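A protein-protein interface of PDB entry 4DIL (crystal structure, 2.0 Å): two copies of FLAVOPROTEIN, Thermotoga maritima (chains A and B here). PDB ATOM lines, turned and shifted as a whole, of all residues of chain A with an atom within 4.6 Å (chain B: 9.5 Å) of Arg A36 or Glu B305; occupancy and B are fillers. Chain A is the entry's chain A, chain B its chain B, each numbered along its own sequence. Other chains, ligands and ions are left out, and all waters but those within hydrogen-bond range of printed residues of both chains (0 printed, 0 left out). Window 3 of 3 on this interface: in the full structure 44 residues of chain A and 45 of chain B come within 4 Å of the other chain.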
ATOM      1  N   PRO A  14     -15.733  28.565  37.548  1.00  0.00           N
ATOM      2  CA  PRO A  14     -15.174  27.437  38.305  1.00  0.00           C
ATOM      3  C   PRO A  14     -15.772  27.417  39.702  1.00  0.00           C
ATOM      4  O   PRO A  14     -16.192  28.473  40.187  1.00  0.00           O
ATOM      5  CB  PRO A  14     -13.682  27.771  38.381  1.00  0.00           C
ATOM      6  CG  PRO A  14     -13.426  28.615  37.160  1.00  0.00           C
ATOM      7  CD  PRO A  14     -14.670  29.472  37.069  1.00  0.00           C
ATOM      8  N   ASP A  34      -9.834  24.639  39.345  1.00  0.00           N
ATOM      9  CA  ASP A  34      -9.502  24.962  37.967  1.00  0.00           C
ATOM     10  C   ASP A  34      -9.912  23.823  37.053  1.00  0.00           C
ATOM     11  O   ASP A  34      -9.206  22.811  36.953  1.00  0.00           O
ATOM     12  CB  ASP A  34      -7.994  25.199  37.838  1.00  0.00           C
ATOM     13  CG  ASP A  34      -7.629  25.946  36.580  1.00  0.00           C
ATOM     14  OD1 ASP A  34      -8.494  26.038  35.691  1.00  0.00           O
ATOM     15  OD2 ASP A  34      -6.484  26.446  36.484  1.00  0.00           O
ATOM     16  N   ASP A  35     -11.059  23.967  36.400  1.00  0.00           N
ATOM     17  CA  ASP A  35     -11.496  22.967  35.431  1.00  0.00           C
ATOM     18  C   ASP A  35     -11.286  23.496  34.016  1.00  0.00           C
ATOM     19  O   ASP A  35     -11.752  22.910  33.042  1.00  0.00           O
ATOM     20  CB  ASP A  35     -12.956  22.544  35.668  1.00  0.00           C
ATOM     21  CG  ASP A  35     -13.939  23.711  35.622  1.00  0.00           C
ATOM     22  OD1 ASP A  35     -13.531  24.863  35.376  1.00  0.00           O
ATOM     23  OD2 ASP A  35     -15.147  23.461  35.830  1.00  0.00           O
ATOM     24  N   ARG A  36     -10.566  24.611  33.928  1.00  0.00           N
ATOM     25  CA  ARG A  36     -10.211  25.233  32.660  1.00  0.00           C
ATOM     26  C   ARG A  36      -8.929  24.605  32.137  1.00  0.00           C
ATOM     27  O   ARG A  36      -8.810  24.261  30.958  1.00  0.00           O
ATOM     28  CB  ARG A  36      -9.947  26.721  32.901  1.00  0.00           C
ATOM     29  CG  ARG A  36     -10.551  27.649  31.891  1.00  0.00           C
ATOM     30  CD  ARG A  36     -11.669  28.453  32.533  1.00  0.00           C
ATOM     31  NE  ARG A  36     -11.367  29.880  32.603  1.00  0.00           N
ATOM     32  CZ  ARG A  36     -12.127  30.774  33.237  1.00  0.00           C
ATOM     33  NH1 ARG A  36     -13.232  30.385  33.859  1.00  0.00           N
ATOM     34  NH2 ARG A  36     -11.784  32.061  33.247  1.00  0.00           N
ATOM     35  N   ILE A  37      -7.967  24.467  33.046  1.00  0.00           N
ATOM     36  CA  ILE A  37      -6.623  24.017  32.719  1.00  0.00           C
ATOM     37  C   ILE A  37      -6.647  22.633  32.074  1.00  0.00           C
ATOM     38  O   ILE A  37      -7.495  21.803  32.395  1.00  0.00           O
ATOM     39  CB  ILE A  37      -5.737  24.042  33.994  1.00  0.00           C
ATOM     40  CG1 ILE A  37      -4.262  23.799  33.672  1.00  0.00           C
ATOM     41  CG2 ILE A  37      -6.247  23.059  35.061  1.00  0.00           C
ATOM     42  CD1 ILE A  37      -3.326  24.327  34.794  1.00  0.00           C
ATOM     43  N   ARG A  38      -5.742  22.401  31.130  1.00  0.00           N
ATOM     44  CA  ARG A  38      -5.630  21.094  30.503  1.00  0.00           C
ATOM     45  C   ARG A  38      -4.242  20.498  30.705  1.00  0.00           C
ATOM     46  O   ARG A  38      -4.094  19.280  30.745  1.00  0.00           O
ATOM     47  CB  ARG A  38      -5.957  21.164  29.005  1.00  0.00           C
ATOM     48  CG  ARG A  38      -7.267  21.873  28.662  1.00  0.00           C
ATOM     49  CD  ARG A  38      -7.536  21.839  27.150  1.00  0.00           C
ATOM     50  NE  ARG A  38      -7.894  20.493  26.714  1.00  0.00           N
ATOM     51  CZ  ARG A  38      -7.486  19.922  25.585  1.00  0.00           C
ATOM     52  NH1 ARG A  38      -6.699  20.580  24.742  1.00  0.00           N
ATOM     53  NH2 ARG A  38      -7.871  18.683  25.302  1.00  0.00           N
ATOM     54  N   TYR A  39      -3.230  21.352  30.828  1.00  0.00           N
ATOM     55  CA  TYR A  39      -1.848  20.874  30.973  1.00  0.00           C
ATOM     56  C   TYR A  39      -1.110  21.628  32.066  1.00  0.00           C
ATOM     57  O   TYR A  39      -0.818  22.819  31.925  1.00  0.00           O
ATOM     58  CB  TYR A  39      -1.064  21.010  29.661  1.00  0.00           C
ATOM     59  CG  TYR A  39      -1.791  20.476  28.458  1.00  0.00           C
ATOM     60  CD1 TYR A  39      -1.949  19.110  28.275  1.00  0.00           C
ATOM     61  CD2 TYR A  39      -2.335  21.338  27.514  1.00  0.00           C
ATOM     62  CE1 TYR A  39      -2.627  18.603  27.172  1.00  0.00           C
ATOM     63  CE2 TYR A  39      -3.010  20.849  26.409  1.00  0.00           C
ATOM     64  CZ  TYR A  39      -3.154  19.481  26.247  1.00  0.00           C
ATOM     65  OH  TYR A  39      -3.823  18.983  25.157  1.00  0.00           O
ATOM     66  N   ASN A  72      -4.886  34.170  36.346  1.00  0.00           N
ATOM     67  CA  ASN A  72      -6.108  34.374  35.584  1.00  0.00           C
ATOM     68  C   ASN A  72      -7.365  34.364  36.462  1.00  0.00           C
ATOM     69  O   ASN A  72      -8.454  34.692  35.997  1.00  0.00           O
ATOM     70  CB  ASN A  72      -6.212  33.390  34.409  1.00  0.00           C
ATOM     71  CG  ASN A  72      -6.176  31.937  34.855  1.00  0.00           C
ATOM     72  OD1 ASN A  72      -5.541  31.603  35.853  1.00  0.00           O
ATOM     73  ND2 ASN A  72      -6.853  31.063  34.109  1.00  0.00           N
ATOM     74  N   TYR A  73      -7.211  34.010  37.738  1.00  0.00           N
ATOM     75  CA  TYR A  73      -8.339  33.985  38.661  1.00  0.00           C
ATOM     76  C   TYR A  73      -8.230  35.052  39.737  1.00  0.00           C
ATOM     77  O   TYR A  73      -8.896  34.978  40.765  1.00  0.00           O
ATOM     78  CB  TYR A  73      -8.455  32.603  39.302  1.00  0.00           C
ATOM     79  CG  TYR A  73      -8.819  31.531  38.311  1.00  0.00           C
ATOM     80  CD1 TYR A  73      -9.885  31.701  37.440  1.00  0.00           C
ATOM     81  CD2 TYR A  73      -8.090  30.352  38.238  1.00  0.00           C
ATOM     82  CE1 TYR A  73     -10.230  30.715  36.539  1.00  0.00           C
ATOM     83  CE2 TYR A  73      -8.419  29.364  37.330  1.00  0.00           C
ATOM     84  CZ  TYR A  73      -9.492  29.552  36.480  1.00  0.00           C
ATOM     85  OH  TYR A  73      -9.831  28.573  35.571  1.00  0.00           O
ATOM     86  N   SER B 274       4.688  28.778  27.193  1.00  0.00           N
ATOM     87  CA  SER B 274       4.390  29.781  28.188  1.00  0.00           C
ATOM     88  C   SER B 274       3.810  29.078  29.410  1.00  0.00           C
ATOM     89  O   SER B 274       2.617  28.805  29.466  1.00  0.00           O
ATOM     90  CB  SER B 274       3.418  30.803  27.611  1.00  0.00           C
ATOM     91  OG  SER B 274       3.198  31.861  28.520  1.00  0.00           O
ATOM     92  N   MET B 275       4.672  28.764  30.373  1.00  0.00           N
ATOM     93  CA  MET B 275       4.242  28.050  31.569  1.00  0.00           C
ATOM     94  C   MET B 275       3.329  28.896  32.460  1.00  0.00           C
ATOM     95  O   MET B 275       2.361  28.372  33.005  1.00  0.00           O
ATOM     96  CB  MET B 275       5.456  27.543  32.363  1.00  0.00           C
ATOM     97  CG  MET B 275       5.871  26.081  32.098  1.00  0.00           C
ATOM     98  SD  MET B 275       7.663  25.822  32.323  1.00  0.00           S
ATOM     99  CE  MET B 275       8.041  27.240  33.326  1.00  0.00           C
ATOM    100  N   LYS B 301       2.054  27.999  20.199  1.00  0.00           N
ATOM    101  CA  LYS B 301       2.145  28.290  21.617  1.00  0.00           C
ATOM    102  C   LYS B 301       1.775  27.074  22.448  1.00  0.00           C
ATOM    103  O   LYS B 301       0.661  26.553  22.331  1.00  0.00           O
ATOM    104  CB  LYS B 301       1.203  29.449  21.949  1.00  0.00           C
ATOM    105  CG  LYS B 301       1.061  29.781  23.421  1.00  0.00           C
ATOM    106  CD  LYS B 301       0.012  30.887  23.569  1.00  0.00           C
ATOM    107  CE  LYS B 301      -0.518  31.002  24.972  1.00  0.00           C
ATOM    108  NZ  LYS B 301      -1.702  31.916  25.036  1.00  0.00           N
ATOM    109  N   PHE B 302       2.717  26.626  23.276  1.00  0.00           N
ATOM    110  CA  PHE B 302       2.447  25.595  24.269  1.00  0.00           C
ATOM    111  C   PHE B 302       2.048  26.293  25.569  1.00  0.00           C
ATOM    112  O   PHE B 302       2.871  26.957  26.194  1.00  0.00           O
ATOM    113  CB  PHE B 302       3.689  24.725  24.535  1.00  0.00           C
ATOM    114  CG  PHE B 302       4.161  23.927  23.341  1.00  0.00           C
ATOM    115  CD1 PHE B 302       3.632  22.667  23.075  1.00  0.00           C
ATOM    116  CD2 PHE B 302       5.149  24.428  22.498  1.00  0.00           C
ATOM    117  CE1 PHE B 302       4.061  21.926  21.974  1.00  0.00           C
ATOM    118  CE2 PHE B 302       5.591  23.697  21.387  1.00  0.00           C
ATOM    119  CZ  PHE B 302       5.047  22.435  21.127  1.00  0.00           C
ATOM    120  N   SER B 303       0.794  26.136  25.975  1.00  0.00           N
ATOM    121  CA  SER B 303       0.307  26.755  27.208  1.00  0.00           C
ATOM    122  C   SER B 303      -0.406  25.715  28.061  1.00  0.00           C
ATOM    123  O   SER B 303      -0.438  24.539  27.695  1.00  0.00           O
ATOM    124  CB  SER B 303      -0.684  27.850  26.879  1.00  0.00           C
ATOM    125  OG  SER B 303      -1.844  27.266  26.343  1.00  0.00           O
ATOM    126  N   ASP B 304      -1.009  26.150  29.166  1.00  0.00           N
ATOM    127  CA  ASP B 304      -1.756  25.226  30.012  1.00  0.00           C
ATOM    128  C   ASP B 304      -3.144  24.898  29.456  1.00  0.00           C
ATOM    129  O   ASP B 304      -3.840  24.039  29.991  1.00  0.00           O
ATOM    130  CB  ASP B 304      -1.818  25.696  31.483  1.00  0.00           C
ATOM    131  CG  ASP B 304      -2.377  27.101  31.639  1.00  0.00           C
ATOM    132  OD1 ASP B 304      -3.093  27.568  30.730  1.00  0.00           O
ATOM    133  OD2 ASP B 304      -2.102  27.743  32.680  1.00  0.00           O
ATOM    134  N   GLU B 305      -3.521  25.542  28.357  1.00  0.00           N
ATOM    135  CA  GLU B 305      -4.840  25.325  27.760  1.00  0.00           C
ATOM    136  C   GLU B 305      -4.752  24.721  26.369  1.00  0.00           C
ATOM    137  O   GLU B 305      -5.647  24.007  25.924  1.00  0.00           O
ATOM    138  CB  GLU B 305      -5.615  26.647  27.669  1.00  0.00           C
ATOM    139  CG  GLU B 305      -5.549  27.495  28.917  1.00  0.00           C
ATOM    140  CD  GLU B 305      -6.922  27.862  29.450  1.00  0.00           C
ATOM    141  OE1 GLU B 305      -7.885  27.860  28.649  1.00  0.00           O
ATOM    142  OE2 GLU B 305      -7.035  28.144  30.673  1.00  0.00           O
ATOM    143  N   GLU B 306      -3.682  25.026  25.659  1.00  0.00           N
ATOM    144  CA  GLU B 306      -3.603  24.590  24.270  1.00  0.00           C
ATOM    145  C   GLU B 306      -2.274  23.937  23.917  1.00  0.00           C
ATOM    146  O   GLU B 306      -1.242  24.239  24.519  1.00  0.00           O
ATOM    147  CB  GLU B 306      -3.922  25.752  23.317  1.00  0.00           C
ATOM    148  CG  GLU B 306      -3.035  26.978  23.480  1.00  0.00           C
ATOM    149  CD  GLU B 306      -3.704  28.251  22.963  1.00  0.00           C
ATOM    150  OE1 GLU B 306      -3.278  28.770  21.907  1.00  0.00           O
ATOM    151  OE2 GLU B 306      -4.655  28.734  23.621  1.00  0.00           O
ATOM    152  N   ARG B 307      -2.315  23.047  22.929  1.00  0.00           N
ATOM    153  CA  ARG B 307      -1.132  22.319  22.500  1.00  0.00           C
ATOM    154  C   ARG B 307      -1.094  22.065  21.003  1.00  0.00           C
ATOM    155  O   ARG B 307      -1.832  21.209  20.499  1.00  0.00           O
ATOM    156  CB  ARG B 307      -1.059  20.984  23.213  1.00  0.00           C
ATOM    157  CG  ARG B 307       0.272  20.805  23.859  1.00  0.00           C
ATOM    158  CD  ARG B 307       1.068  19.669  23.289  1.00  0.00           C
ATOM    159  NE  ARG B 307       0.871  18.390  23.983  1.00  0.00           N
ATOM    160  CZ  ARG B 307       0.816  18.194  25.305  1.00  0.00           C
ATOM    161  NH1 ARG B 307       0.913  19.187  26.191  1.00  0.00           N
ATOM    162  NH2 ARG B 307       0.649  16.962  25.751  1.00  0.00           N
ATOM    163  N   PRO B 308      -0.201  22.780  20.295  1.00  0.00           N
ATOM    164  CA  PRO B 308      -0.074  22.668  18.840  1.00  0.00           C
ATOM    165  C   PRO B 308       0.389  21.277  18.427  1.00  0.00           C
ATOM    166  O   PRO B 308       1.093  20.610  19.182  1.00  0.00           O
ATOM    167  CB  PRO B 308       1.015  23.692  18.506  1.00  0.00           C
ATOM    168  CG  PRO B 308       1.789  23.860  19.772  1.00  0.00           C
ATOM    169  CD  PRO B 308       0.778  23.721  20.864  1.00  0.00           C
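No position is printed for both chains.
N of Arg A36 sits at hydrogen-bond distance from OD1 of Asp A34, at 3.1 Å.
N of Ile A37 lies within hydrogen-bond range of OD1 of Asp A34 (3.1 Å).
NH1 of Arg A38 lies within hydrogen-bond range of OH of Tyr A39 (3.3 Å).
The backbone NH (N) of Glu B305 lies close to the side-chain hydroxyl (OG) of Ser B303.
The side-chain hydroxyl of Ser B303 is in hydrogen-bond range of the backbone NH of Glu B306, 3.0 Å away.
The backbone carbonyl oxygen of Asp B304 sits at hydrogen-bond distance from the backbone NH of Arg A38, at 2.8 Å.
The backbone carbonyl oxygen (O) of Asp B304 is in hydrogen-bond range of the backbone NH (N) of Tyr A39 (2.9 Å).
Of the 9 printed residues of chain A, 4 touch a printed residue of chain B.
Printed residues of chain B that touch a printed residue of chain A: Ser B303, Asp B304, Glu B305 and Arg B307.
Among the printed residues, 7 pairs touch across the chains.
Among the printed residues, no Asp or Glu carboxylate lies within 4 Å of a Lys or Arg side-chain nitrogen of the other chain.
Among the printed residues, merely in contact across the chains: Arg A36 with Glu B305 (3.8 Å), Ile A37 with Asp B304 (3.7 Å), Arg A38 with Glu B305 (3.1 Å), Tyr A39 with Ser B303 (3.7 Å) and Tyr A39 with Arg B307 (3.5 Å).
Arg A36 touches just one residue of chain B: Glu B305 (3.8 Å).
Of the printed residues of chain B, Ile A37 touches Asp B304.
Of the printed residues of chain B, Arg A38 touches Asp B304 (2.8 Å) and Glu B305 (3.1 Å).
Printed residues of chain A within 4 Å of Ser B303: Tyr A39 (3.7 Å).
Of the printed residues of chain A, Asp B304 touches Ile A37, Arg A38 and Tyr A39.
Glu B305 touches two residues of chain A.
Glu B306 touches none of the printed residues of chain A.
The nearest printed residue of chain A that does not touch Arg B307 is Arg A38 (5.3 Å).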
